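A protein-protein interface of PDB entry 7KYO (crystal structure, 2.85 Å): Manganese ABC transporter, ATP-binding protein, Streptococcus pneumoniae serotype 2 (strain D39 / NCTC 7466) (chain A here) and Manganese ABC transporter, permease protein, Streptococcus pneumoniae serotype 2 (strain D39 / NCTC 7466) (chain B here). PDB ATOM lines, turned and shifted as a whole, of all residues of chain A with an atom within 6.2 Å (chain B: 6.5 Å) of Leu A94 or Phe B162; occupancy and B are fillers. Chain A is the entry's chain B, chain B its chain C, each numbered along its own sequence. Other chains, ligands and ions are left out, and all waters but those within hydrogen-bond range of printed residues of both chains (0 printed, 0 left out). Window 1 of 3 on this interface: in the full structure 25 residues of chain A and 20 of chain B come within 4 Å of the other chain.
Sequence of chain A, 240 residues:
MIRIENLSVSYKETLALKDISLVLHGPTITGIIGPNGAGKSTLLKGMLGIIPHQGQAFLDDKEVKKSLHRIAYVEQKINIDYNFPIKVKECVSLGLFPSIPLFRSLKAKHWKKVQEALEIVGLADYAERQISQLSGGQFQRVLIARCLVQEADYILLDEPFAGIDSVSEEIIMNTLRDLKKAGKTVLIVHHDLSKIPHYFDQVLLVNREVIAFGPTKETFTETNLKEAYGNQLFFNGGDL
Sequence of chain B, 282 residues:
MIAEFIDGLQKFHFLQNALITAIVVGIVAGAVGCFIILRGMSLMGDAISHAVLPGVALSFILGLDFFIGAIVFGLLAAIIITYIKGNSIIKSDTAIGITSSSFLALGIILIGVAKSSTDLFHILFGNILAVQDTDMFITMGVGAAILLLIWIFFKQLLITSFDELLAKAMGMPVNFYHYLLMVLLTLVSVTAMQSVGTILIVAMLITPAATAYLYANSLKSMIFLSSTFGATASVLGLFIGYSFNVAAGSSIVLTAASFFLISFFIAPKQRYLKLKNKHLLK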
ATOM      1  N   GLU A  75     -22.100   5.641  -5.099  1.00  0.00           N
ATOM      2  CA  GLU A  75     -22.813   4.390  -4.837  1.00  0.00           C
ATOM      3  C   GLU A  75     -23.491   3.862  -6.094  1.00  0.00           C
ATOM      4  O   GLU A  75     -23.499   4.521  -7.137  1.00  0.00           O
ATOM      5  CB  GLU A  75     -23.846   4.581  -3.722  1.00  0.00           C
ATOM      6  CG  GLU A  75     -25.100   5.346  -4.134  1.00  0.00           C
ATOM      7  CD  GLU A  75     -25.665   6.192  -3.014  1.00  0.00           C
ATOM      8  OE1 GLU A  75     -24.973   7.157  -2.613  1.00  0.00           O
ATOM      9  OE2 GLU A  75     -26.793   5.903  -2.547  1.00  0.00           O
ATOM     10  N   ASN A  79     -29.873   1.889  -5.459  1.00  0.00           N
ATOM     11  CA  ASN A  79     -30.400   2.221  -4.114  1.00  0.00           C
ATOM     12  C   ASN A  79     -30.626   3.727  -3.870  1.00  0.00           C
ATOM     13  O   ASN A  79     -30.536   4.198  -2.738  1.00  0.00           O
ATOM     14  CB  ASN A  79     -29.559   1.562  -2.991  1.00  0.00           C
ATOM     15  CG  ASN A  79     -28.107   2.012  -2.970  1.00  0.00           C
ATOM     16  OD1 ASN A  79     -27.783   3.158  -3.268  1.00  0.00           O
ATOM     17  ND2 ASN A  79     -27.222   1.100  -2.593  1.00  0.00           N
ATOM     18  N   ILE A  80     -30.931   4.466  -4.935  1.00  0.00           N
ATOM     19  CA  ILE A  80     -31.388   5.856  -4.837  1.00  0.00           C
ATOM     20  C   ILE A  80     -32.829   5.903  -5.346  1.00  0.00           C
ATOM     21  O   ILE A  80     -33.142   5.337  -6.400  1.00  0.00           O
ATOM     22  CB  ILE A  80     -30.500   6.817  -5.667  1.00  0.00           C
ATOM     23  CG1 ILE A  80     -29.069   6.831  -5.117  1.00  0.00           C
ATOM     24  CG2 ILE A  80     -31.074   8.233  -5.665  1.00  0.00           C
ATOM     25  CD1 ILE A  80     -28.056   7.473  -6.043  1.00  0.00           C
ATOM     26  N   ASP A  81     -33.699   6.578  -4.597  1.00  0.00           N
ATOM     27  CA  ASP A  81     -35.087   6.761  -5.009  1.00  0.00           C
ATOM     28  C   ASP A  81     -35.132   7.818  -6.110  1.00  0.00           C
ATOM     29  O   ASP A  81     -34.911   9.002  -5.852  1.00  0.00           O
ATOM     30  CB  ASP A  81     -35.964   7.171  -3.818  1.00  0.00           C
ATOM     31  CG  ASP A  81     -37.457   7.212  -4.158  1.00  0.00           C
ATOM     32  OD1 ASP A  81     -37.875   6.662  -5.204  1.00  0.00           O
ATOM     33  OD2 ASP A  81     -38.221   7.797  -3.359  1.00  0.00           O
ATOM     34  N   TYR A  82     -35.418   7.366  -7.331  1.00  0.00           N
ATOM     35  CA  TYR A  82     -35.504   8.228  -8.519  1.00  0.00           C
ATOM     36  C   TYR A  82     -36.691   9.196  -8.434  1.00  0.00           C
ATOM     37  O   TYR A  82     -36.650  10.296  -8.984  1.00  0.00           O
ATOM     38  CB  TYR A  82     -35.644   7.377  -9.793  1.00  0.00           C
ATOM     39  CG  TYR A  82     -34.391   6.636 -10.218  1.00  0.00           C
ATOM     40  CD1 TYR A  82     -33.992   5.463  -9.585  1.00  0.00           C
ATOM     41  CD2 TYR A  82     -33.619   7.101 -11.272  1.00  0.00           C
ATOM     42  CE1 TYR A  82     -32.853   4.789  -9.980  1.00  0.00           C
ATOM     43  CE2 TYR A  82     -32.483   6.429 -11.677  1.00  0.00           C
ATOM     44  CZ  TYR A  82     -32.102   5.277 -11.025  1.00  0.00           C
ATOM     45  OH  TYR A  82     -30.969   4.610 -11.426  1.00  0.00           O
ATOM     46  N   PHE A  84     -37.812  10.717  -5.747  1.00  0.00           N
ATOM     47  CA  PHE A  84     -37.602  11.794  -4.767  1.00  0.00           C
ATOM     48  C   PHE A  84     -37.641  13.145  -5.497  1.00  0.00           C
ATOM     49  O   PHE A  84     -37.064  13.261  -6.579  1.00  0.00           O
ATOM     50  CB  PHE A  84     -36.250  11.611  -4.054  1.00  0.00           C
ATOM     51  CG  PHE A  84     -36.052  12.515  -2.863  1.00  0.00           C
ATOM     52  CD1 PHE A  84     -35.552  13.807  -3.022  1.00  0.00           C
ATOM     53  CD2 PHE A  84     -36.354  12.072  -1.577  1.00  0.00           C
ATOM     54  CE1 PHE A  84     -35.374  14.642  -1.927  1.00  0.00           C
ATOM     55  CE2 PHE A  84     -36.174  12.902  -0.478  1.00  0.00           C
ATOM     56  CZ  PHE A  84     -35.683  14.188  -0.653  1.00  0.00           C
ATOM     57  N   ILE A  86     -36.304  16.112  -6.579  1.00  0.00           N
ATOM     58  CA  ILE A  86     -34.999  16.776  -6.620  1.00  0.00           C
ATOM     59  C   ILE A  86     -34.523  16.953  -8.065  1.00  0.00           C
ATOM     60  O   ILE A  86     -34.661  16.046  -8.890  1.00  0.00           O
ATOM     61  CB  ILE A  86     -33.948  16.015  -5.766  1.00  0.00           C
ATOM     62  CG1 ILE A  86     -32.634  16.797  -5.682  1.00  0.00           C
ATOM     63  CG2 ILE A  86     -33.699  14.605  -6.293  1.00  0.00           C
ATOM     64  CD1 ILE A  86     -31.723  16.329  -4.568  1.00  0.00           C
ATOM     65  N   LYS A  89     -29.487  19.861 -10.949  1.00  0.00           N
ATOM     66  CA  LYS A  89     -28.673  20.919 -10.338  1.00  0.00           C
ATOM     67  C   LYS A  89     -28.554  20.738  -8.822  1.00  0.00           C
ATOM     68  O   LYS A  89     -27.452  20.791  -8.275  1.00  0.00           O
ATOM     69  CB  LYS A  89     -29.274  22.299 -10.661  1.00  0.00           C
ATOM     70  CG  LYS A  89     -28.446  23.497 -10.211  1.00  0.00           C
ATOM     71  CD  LYS A  89     -29.084  24.809 -10.649  1.00  0.00           C
ATOM     72  CE  LYS A  89     -28.443  26.002  -9.948  1.00  0.00           C
ATOM     73  NZ  LYS A  89     -29.060  27.305 -10.332  1.00  0.00           N
ATOM     74  N   GLU A  90     -29.688  20.517  -8.160  1.00  0.00           N
ATOM     75  CA  GLU A  90     -29.721  20.298  -6.708  1.00  0.00           C
ATOM     76  C   GLU A  90     -29.024  18.998  -6.303  1.00  0.00           C
ATOM     77  O   GLU A  90     -28.347  18.955  -5.274  1.00  0.00           O
ATOM     78  CB  GLU A  90     -31.163  20.302  -6.181  1.00  0.00           C
ATOM     79  CG  GLU A  90     -31.271  20.315  -4.658  1.00  0.00           C
ATOM     80  CD  GLU A  90     -32.684  20.573  -4.154  1.00  0.00           C
ATOM     81  OE1 GLU A  90     -33.658  20.196  -4.846  1.00  0.00           O
ATOM     82  OE2 GLU A  90     -32.821  21.150  -3.050  1.00  0.00           O
ATOM     83  N   CYS A  91     -29.194  17.950  -7.110  1.00  0.00           N
ATOM     84  CA  CYS A  91     -28.563  16.653  -6.845  1.00  0.00           C
ATOM     85  C   CYS A  91     -27.037  16.744  -6.867  1.00  0.00           C
ATOM     86  O   CYS A  91     -26.375  16.204  -5.983  1.00  0.00           O
ATOM     87  CB  CYS A  91     -29.034  15.601  -7.851  1.00  0.00           C
ATOM     88  SG  CYS A  91     -28.534  13.919  -7.426  1.00  0.00           S
ATOM     89  N   VAL A  92     -26.494  17.440  -7.866  1.00  0.00           N
ATOM     90  CA  VAL A  92     -25.046  17.666  -7.971  1.00  0.00           C
ATOM     91  C   VAL A  92     -24.525  18.529  -6.813  1.00  0.00           C
ATOM     92  O   VAL A  92     -23.424  18.286  -6.314  1.00  0.00           O
ATOM     93  CB  VAL A  92     -24.657  18.277  -9.343  1.00  0.00           C
ATOM     94  CG1 VAL A  92     -23.193  18.714  -9.378  1.00  0.00           C
ATOM     95  CG2 VAL A  92     -24.924  17.267 -10.451  1.00  0.00           C
ATOM     96  N   SER A  93     -25.320  19.506  -6.372  1.00  0.00           N
ATOM     97  CA  SER A  93     -24.928  20.387  -5.259  1.00  0.00           C
ATOM     98  C   SER A  93     -24.789  19.678  -3.901  1.00  0.00           C
ATOM     99  O   SER A  93     -24.187  20.234  -2.983  1.00  0.00           O
ATOM    100  CB  SER A  93     -25.895  21.569  -5.126  1.00  0.00           C
ATOM    101  OG  SER A  93     -27.130  21.172  -4.557  1.00  0.00           O
ATOM    102  N   LEU A  94     -25.343  18.468  -3.779  1.00  0.00           N
ATOM    103  CA  LEU A  94     -25.189  17.637  -2.573  1.00  0.00           C
ATOM    104  C   LEU A  94     -23.733  17.282  -2.241  1.00  0.00           C
ATOM    105  O   LEU A  94     -23.414  17.032  -1.079  1.00  0.00           O
ATOM    106  CB  LEU A  94     -26.000  16.338  -2.692  1.00  0.00           C
ATOM    107  CG  LEU A  94     -27.520  16.421  -2.870  1.00  0.00           C
ATOM    108  CD1 LEU A  94     -28.113  15.025  -2.882  1.00  0.00           C
ATOM    109  CD2 LEU A  94     -28.169  17.270  -1.789  1.00  0.00           C
ATOM    110  N   GLY A  95     -22.861  17.249  -3.250  1.00  0.00           N
ATOM    111  CA  GLY A  95     -21.424  17.047  -3.041  1.00  0.00           C
ATOM    112  C   GLY A  95     -20.761  18.114  -2.188  1.00  0.00           C
ATOM    113  O   GLY A  95     -19.802  17.829  -1.474  1.00  0.00           O
ATOM    114  N   LEU A  96     -21.286  19.337  -2.251  1.00  0.00           N
ATOM    115  CA  LEU A  96     -20.759  20.479  -1.494  1.00  0.00           C
ATOM    116  C   LEU A  96     -21.419  20.698  -0.119  1.00  0.00           C
ATOM    117  O   LEU A  96     -21.098  21.669   0.565  1.00  0.00           O
ATOM    118  CB  LEU A  96     -20.898  21.746  -2.345  1.00  0.00           C
ATOM    119  CG  LEU A  96     -20.159  21.686  -3.688  1.00  0.00           C
ATOM    120  CD1 LEU A  96     -20.665  22.725  -4.679  1.00  0.00           C
ATOM    121  CD2 LEU A  96     -18.657  21.834  -3.478  1.00  0.00           C
ATOM    122  N   PHE A  97     -22.327  19.807   0.284  1.00  0.00           N
ATOM    123  CA  PHE A  97     -23.043  19.926   1.568  1.00  0.00           C
ATOM    124  C   PHE A  97     -22.174  19.812   2.837  1.00  0.00           C
ATOM    125  O   PHE A  97     -22.506  20.435   3.846  1.00  0.00           O
ATOM    126  CB  PHE A  97     -24.217  18.921   1.634  1.00  0.00           C
ATOM    127  CG  PHE A  97     -25.507  19.418   1.011  1.00  0.00           C
ATOM    128  CD1 PHE A  97     -25.516  20.344  -0.039  1.00  0.00           C
ATOM    129  CD2 PHE A  97     -26.732  18.936   1.471  1.00  0.00           C
ATOM    130  CE1 PHE A  97     -26.710  20.783  -0.589  1.00  0.00           C
ATOM    131  CE2 PHE A  97     -27.927  19.373   0.918  1.00  0.00           C
ATOM    132  CZ  PHE A  97     -27.917  20.298  -0.111  1.00  0.00           C
ATOM    133  N   PRO A  98     -21.090  19.005   2.811  1.00  0.00           N
ATOM    134  CA  PRO A  98     -20.169  19.055   3.961  1.00  0.00           C
ATOM    135  C   PRO A  98     -19.336  20.344   4.039  1.00  0.00           C
ATOM    136  O   PRO A  98     -18.995  20.778   5.141  1.00  0.00           O
ATOM    137  CB  PRO A  98     -19.266  17.828   3.756  1.00  0.00           C
ATOM    138  CG  PRO A  98     -19.427  17.446   2.330  1.00  0.00           C
ATOM    139  CD  PRO A  98     -20.819  17.839   1.953  1.00  0.00           C
ATOM    140  N   ILE A 131     -34.636  14.120 -11.651  1.00  0.00           N
ATOM    141  CA  ILE A 131     -33.794  12.928 -11.835  1.00  0.00           C
ATOM    142  C   ILE A 131     -34.578  11.714 -12.378  1.00  0.00           C
ATOM    143  O   ILE A 131     -34.004  10.872 -13.070  1.00  0.00           O
ATOM    144  CB  ILE A 131     -32.991  12.563 -10.558  1.00  0.00           C
ATOM    145  CG1 ILE A 131     -33.905  12.258  -9.365  1.00  0.00           C
ATOM    146  CG2 ILE A 131     -32.023  13.686 -10.209  1.00  0.00           C
ATOM    147  CD1 ILE A 131     -33.180  11.652  -8.183  1.00  0.00           C
ATOM    148  N   PHE A 139     -28.375   9.603 -15.487  1.00  0.00           N
ATOM    149  CA  PHE A 139     -28.402   9.672 -14.022  1.00  0.00           C
ATOM    150  C   PHE A 139     -27.051   9.291 -13.417  1.00  0.00           C
ATOM    151  O   PHE A 139     -26.640   9.870 -12.414  1.00  0.00           O
ATOM    152  CB  PHE A 139     -29.519   8.794 -13.437  1.00  0.00           C
ATOM    153  CG  PHE A 139     -29.636   8.877 -11.932  1.00  0.00           C
ATOM    154  CD1 PHE A 139     -29.795  10.110 -11.297  1.00  0.00           C
ATOM    155  CD2 PHE A 139     -29.583   7.730 -11.143  1.00  0.00           C
ATOM    156  CE1 PHE A 139     -29.897  10.197  -9.915  1.00  0.00           C
ATOM    157  CE2 PHE A 139     -29.693   7.813  -9.760  1.00  0.00           C
ATOM    158  CZ  PHE A 139     -29.847   9.046  -9.145  1.00  0.00           C
ATOM    159  N   LEU A 143     -24.378  11.550 -10.913  1.00  0.00           N
ATOM    160  CA  LEU A 143     -23.628  11.068  -9.749  1.00  0.00           C
ATOM    161  C   LEU A 143     -22.120  11.296  -9.887  1.00  0.00           C
ATOM    162  O   LEU A 143     -21.437  11.521  -8.887  1.00  0.00           O
ATOM    163  CB  LEU A 143     -23.904   9.578  -9.498  1.00  0.00           C
ATOM    164  CG  LEU A 143     -25.349   9.135  -9.250  1.00  0.00           C
ATOM    165  CD1 LEU A 143     -25.395   7.629  -9.048  1.00  0.00           C
ATOM    166  CD2 LEU A 143     -25.964   9.856  -8.059  1.00  0.00           C
ATOM    167  N   ARG A 146     -21.745  15.014  -9.308  1.00  0.00           N
ATOM    168  CA  ARG A 146     -21.852  15.153  -7.847  1.00  0.00           C
ATOM    169  C   ARG A 146     -20.566  14.740  -7.131  1.00  0.00           C
ATOM    170  O   ARG A 146     -20.222  15.293  -6.093  1.00  0.00           O
ATOM    171  CB  ARG A 146     -23.019  14.310  -7.322  1.00  0.00           C
ATOM    172  CG  ARG A 146     -23.341  14.526  -5.853  1.00  0.00           C
ATOM    173  CD  ARG A 146     -24.559  13.724  -5.435  1.00  0.00           C
ATOM    174  NE  ARG A 146     -24.270  12.303  -5.271  1.00  0.00           N
ATOM    175  CZ  ARG A 146     -25.150  11.401  -4.844  1.00  0.00           C
ATOM    176  NH1 ARG A 146     -24.781  10.129  -4.721  1.00  0.00           N
ATOM    177  NH2 ARG A 146     -26.397  11.756  -4.532  1.00  0.00           N
ATOM    178  N   VAL A 149     -17.592  17.661  -7.803  1.00  0.00           N
ATOM    179  CA  VAL A 149     -17.663  18.896  -6.990  1.00  0.00           C
ATOM    180  C   VAL A 149     -17.032  18.796  -5.588  1.00  0.00           C
ATOM    181  O   VAL A 149     -16.680  19.821  -5.000  1.00  0.00           O
ATOM    182  CB  VAL A 149     -19.107  19.455  -6.870  1.00  0.00           C
ATOM    183  CG1 VAL A 149     -19.609  19.931  -8.224  1.00  0.00           C
ATOM    184  CG2 VAL A 149     -20.069  18.438  -6.261  1.00  0.00           C
ATOM    185  N   GLN A 150     -16.894  17.576  -5.061  1.00  0.00           N
ATOM    186  CA  GLN A 150     -16.171  17.346  -3.799  1.00  0.00           C
ATOM    187  C   GLN A 150     -14.674  17.669  -3.860  1.00  0.00           C
ATOM    188  O   GLN A 150     -14.066  17.933  -2.822  1.00  0.00           O
ATOM    189  CB  GLN A 150     -16.335  15.899  -3.326  1.00  0.00           C
ATOM    190  CG  GLN A 150     -17.697  15.580  -2.737  1.00  0.00           C
ATOM    191  CD  GLN A 150     -17.755  14.202  -2.103  1.00  0.00           C
ATOM    192  OE1 GLN A 150     -16.827  13.779  -1.407  1.00  0.00           O
ATOM    193  NE2 GLN A 150     -18.856  13.495  -2.332  1.00  0.00           N
ATOM    194  N   ARG B  39     -39.156   9.136   3.561  1.00  0.00           N
ATOM    195  CA  ARG B  39     -38.394   8.097   4.270  1.00  0.00           C
ATOM    196  C   ARG B  39     -39.160   6.776   4.427  1.00  0.00           C
ATOM    197  O   ARG B  39     -38.552   5.753   4.735  1.00  0.00           O
ATOM    198  CB  ARG B  39     -37.942   8.597   5.647  1.00  0.00           C
ATOM    199  CG  ARG B  39     -36.868   9.670   5.586  1.00  0.00           C
ATOM    200  CD  ARG B  39     -36.788  10.460   6.880  1.00  0.00           C
ATOM    201  NE  ARG B  39     -35.589  11.302   6.934  1.00  0.00           N
ATOM    202  CZ  ARG B  39     -34.426  10.988   7.516  1.00  0.00           C
ATOM    203  NH1 ARG B  39     -34.238   9.822   8.141  1.00  0.00           N
ATOM    204  NH2 ARG B  39     -33.424  11.866   7.478  1.00  0.00           N
ATOM    205  N   LYS B 155     -30.667  21.236   4.851  1.00  0.00           N
ATOM    206  CA  LYS B 155     -29.703  20.547   3.991  1.00  0.00           C
ATOM    207  C   LYS B 155     -29.302  19.166   4.523  1.00  0.00           C
ATOM    208  O   LYS B 155     -29.087  18.240   3.740  1.00  0.00           O
ATOM    209  CB  LYS B 155     -28.456  21.415   3.767  1.00  0.00           C
ATOM    210  CG  LYS B 155     -28.669  22.521   2.746  1.00  0.00           C
ATOM    211  CD  LYS B 155     -27.407  23.344   2.515  1.00  0.00           C
ATOM    212  CE  LYS B 155     -27.230  24.430   3.564  1.00  0.00           C
ATOM    213  NZ  LYS B 155     -28.283  25.481   3.514  1.00  0.00           N
ATOM    214  N   LEU B 157     -31.208  17.255   6.767  1.00  0.00           N
ATOM    215  CA  LEU B 157     -32.429  16.446   6.643  1.00  0.00           C
ATOM    216  C   LEU B 157     -32.749  16.077   5.185  1.00  0.00           C
ATOM    217  O   LEU B 157     -33.370  15.043   4.937  1.00  0.00           O
ATOM    218  CB  LEU B 157     -33.630  17.163   7.277  1.00  0.00           C
ATOM    219  CG  LEU B 157     -33.636  17.294   8.808  1.00  0.00           C
ATOM    220  CD1 LEU B 157     -34.646  18.342   9.255  1.00  0.00           C
ATOM    221  CD2 LEU B 157     -33.918  15.959   9.485  1.00  0.00           C
ATOM    222  N   LEU B 158     -32.339  16.923   4.235  1.00  0.00           N
ATOM    223  CA  LEU B 158     -32.504  16.643   2.798  1.00  0.00           C
ATOM    224  C   LEU B 158     -31.654  15.455   2.357  1.00  0.00           C
ATOM    225  O   LEU B 158     -32.178  14.480   1.809  1.00  0.00           O
ATOM    226  CB  LEU B 158     -32.151  17.880   1.948  1.00  0.00           C
ATOM    227  CG  LEU B 158     -32.029  17.730   0.421  1.00  0.00           C
ATOM    228  CD1 LEU B 158     -33.271  17.103  -0.191  1.00  0.00           C
ATOM    229  CD2 LEU B 158     -31.751  19.077  -0.228  1.00  0.00           C
ATOM    230  N   ILE B 159     -30.347  15.550   2.592  1.00  0.00           N
ATOM    231  CA  ILE B 159     -29.396  14.531   2.132  1.00  0.00           C
ATOM    232  C   ILE B 159     -29.565  13.171   2.818  1.00  0.00           C
ATOM    233  O   ILE B 159     -29.399  12.142   2.173  1.00  0.00           O
ATOM    234  CB  ILE B 159     -27.926  15.009   2.237  1.00  0.00           C
ATOM    235  CG1 ILE B 159     -27.009  14.093   1.424  1.00  0.00           C
ATOM    236  CG2 ILE B 159     -27.452  15.096   3.684  1.00  0.00           C
ATOM    237  CD1 ILE B 159     -25.688  14.731   1.076  1.00  0.00           C
ATOM    238  N   THR B 160     -29.899  13.174   4.109  1.00  0.00           N
ATOM    239  CA  THR B 160     -30.151  11.932   4.849  1.00  0.00           C
ATOM    240  C   THR B 160     -31.465  11.254   4.434  1.00  0.00           C
ATOM    241  O   THR B 160     -31.606  10.041   4.592  1.00  0.00           O
ATOM    242  CB  THR B 160     -30.167  12.163   6.375  1.00  0.00           C
ATOM    243  OG1 THR B 160     -31.149  13.153   6.706  1.00  0.00           O
ATOM    244  CG2 THR B 160     -28.796  12.611   6.877  1.00  0.00           C
ATOM    245  N   SER B 161     -32.418  12.037   3.924  1.00  0.00           N
ATOM    246  CA  SER B 161     -33.672  11.502   3.380  1.00  0.00           C
ATOM    247  C   SER B 161     -33.480  10.911   1.984  1.00  0.00           C
ATOM    248  O   SER B 161     -33.927   9.797   1.712  1.00  0.00           O
ATOM    249  CB  SER B 161     -34.747  12.592   3.321  1.00  0.00           C
ATOM    250  OG  SER B 161     -35.055  13.079   4.616  1.00  0.00           O
ATOM    251  N   PHE B 162     -32.820  11.666   1.107  1.00  0.00           N
ATOM    252  CA  PHE B 162     -32.640  11.273  -0.299  1.00  0.00           C
ATOM    253  C   PHE B 162     -31.574  10.196  -0.488  1.00  0.00           C
ATOM    254  O   PHE B 162     -31.812   9.209  -1.183  1.00  0.00           O
ATOM    255  CB  PHE B 162     -32.298  12.501  -1.154  1.00  0.00           C
ATOM    256  CG  PHE B 162     -31.871  12.175  -2.563  1.00  0.00           C
ATOM    257  CD1 PHE B 162     -32.716  11.483  -3.420  1.00  0.00           C
ATOM    258  CD2 PHE B 162     -30.623  12.577  -3.039  1.00  0.00           C
ATOM    259  CE1 PHE B 162     -32.326  11.192  -4.721  1.00  0.00           C
ATOM    260  CE2 PHE B 162     -30.228  12.289  -4.339  1.00  0.00           C
ATOM    261  CZ  PHE B 162     -31.082  11.598  -5.182  1.00  0.00           C
ATOM    262  N   ASP B 163     -30.405  10.401   0.117  1.00  0.00           N
ATOM    263  CA  ASP B 163     -29.240   9.547  -0.114  1.00  0.00           C
ATOM    264  C   ASP B 163     -28.469   9.307   1.184  1.00  0.00           C
ATOM    265  O   ASP B 163     -27.444   9.941   1.452  1.00  0.00           O
ATOM    266  CB  ASP B 163     -28.348  10.170  -1.193  1.00  0.00           C
ATOM    267  CG  ASP B 163     -27.320   9.200  -1.738  1.00  0.00           C
ATOM    268  OD1 ASP B 163     -26.828   8.351  -0.968  1.00  0.00           O
ATOM    269  OD2 ASP B 163     -26.999   9.286  -2.942  1.00  0.00           O
ATOM    270  N   GLU B 164     -28.981   8.366   1.974  1.00  0.00           N
ATOM    271  CA  GLU B 164     -28.405   8.009   3.271  1.00  0.00           C
ATOM    272  C   GLU B 164     -26.978   7.459   3.172  1.00  0.00           C
ATOM    273  O   GLU B 164     -26.144   7.732   4.032  1.00  0.00           O
ATOM    274  CB  GLU B 164     -29.312   6.990   3.969  1.00  0.00           C
ATOM    275  CG  GLU B 164     -28.843   6.571   5.354  1.00  0.00           C
ATOM    276  CD  GLU B 164     -29.987   6.202   6.286  1.00  0.00           C
ATOM    277  OE1 GLU B 164     -29.995   5.053   6.785  1.00  0.00           O
ATOM    278  OE2 GLU B 164     -30.872   7.064   6.522  1.00  0.00           O
ATOM    279  N   LEU B 166     -24.634   8.140   0.923  1.00  0.00           N
ATOM    280  CA  LEU B 166     -23.713   9.253   0.685  1.00  0.00           C
ATOM    281  C   LEU B 166     -23.429  10.011   1.982  1.00  0.00           C
ATOM    282  O   LEU B 166     -22.274  10.318   2.275  1.00  0.00           O
ATOM    283  CB  LEU B 166     -24.284  10.215  -0.366  1.00  0.00           C
ATOM    284  CG  LEU B 166     -23.427  11.407  -0.816  1.00  0.00           C
ATOM    285  CD1 LEU B 166     -22.148  10.947  -1.506  1.00  0.00           C
ATOM    286  CD2 LEU B 166     -24.235  12.333  -1.720  1.00  0.00           C
ATOM    287  N   MET B 170     -19.808  10.712   3.769  1.00  0.00           N
ATOM    288  CA  MET B 170     -19.289  12.050   4.108  1.00  0.00           C
ATOM    289  C   MET B 170     -19.088  12.265   5.622  1.00  0.00           C
ATOM    290  O   MET B 170     -18.701  13.357   6.049  1.00  0.00           O
ATOM    291  CB  MET B 170     -20.216  13.129   3.536  1.00  0.00           C
ATOM    292  CG  MET B 170     -20.344  13.064   2.016  1.00  0.00           C
ATOM    293  SD  MET B 170     -21.278  14.379   1.198  1.00  0.00           S
ATOM    294  CE  MET B 170     -22.639  14.643   2.329  1.00  0.00           C
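Leu A94 touches just these residues of chain B: Ile B159 and Phe B162. Of the printed residues of chain A, Phe B162 touches Ile A80 (3.3 Å), Asp A81 (3.6 Å), Phe A84 (3.5 Å), Cys A91 (3.9 Å), Leu A94 (3.5 Å), Ile A131 (3.6 Å) and Arg A146 (3.9 Å). Of the printed residues of chain B, Glu A90 touches Leu B158. Of the printed residues of chain B, Pro A98 touches Met B170. Printed residues of chain A within 4 Å of Lys B155: Phe A97. Printed residues of chain B within 4 Å of Cys A91: Phe B162. Printed residues of chain A within 4 Å of Leu B158: Phe A84 (3.7 Å) and Glu A90 (3.7 Å). Asn A79 touches none of the printed residues of chain B. The nearest printed residue of chain B that does not touch Asp A81 is Ser B161 (6.5 Å).
The side-chain amide oxygen (OD1) of Asn A79 lies close to the side-chain carboxylate (OE2) of Glu A75 (3.0 Å). The side-chain carboxylate (OE1) of Glu A75 lies within salt-bridge range of the guanidinium group (NH1) of Arg A146 (3.6 Å). The backbone NH of Ile A131 is in hydrogen-bond range of the backbone carbonyl oxygen of Ile A86, 3.4 Å away. The backbone carbonyl oxygen (O) of Glu A90 is in hydrogen-bond range of the side-chain hydroxyl (OG) of Ser A93 (2.6 Å). N of Leu B166 sits at hydrogen-bond distance from OD1 of Asp B163 (2.9 Å).
Hydrophobic or aromatic side chains of chain A within 4 Å of the printed part of chain B: Ile A80, Phe A84, Leu A94, Phe A97, Pro A98 and Ile A131. Of the 12 printed residues of chain B, 7 touch a printed residue of chain A. Hydrophobic or aromatic side chains of chain B within 4 Å of the printed part of chain A: Leu B158, Ile B159, Phe B162, Leu B166 and Met B170.
The guanidinium group (NH1) of Arg A146 lies within salt-bridge range of the side-chain carboxylate (OD2) of Asp B163, at 3.0 Å. The side-chain carboxylate of Glu A75 sits close to the side-chain carboxylate of Asp B163.
N of Leu B166 touches OE1 of Glu A75, 3.7 Å away. Ile A80 touches Phe B162 (CG2 to CE1, 3.3 Å). Asp B163 touches Ile A80. CE1 of Phe A84 touches CD1 of Leu B158, 3.7 Å away. Leu B158 touches Glu A90 (CD2 to OE2, 3.7 Å). Phe B162 touches Cys A91 (CE2 to SG, 3.9 Å). Ile B159 touches Leu A94. Phe B162 touches Leu A94 (CD2 to CD1, 3.5 Å). Pro A98 touches Met B170. Phe B162 touches Arg A146.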
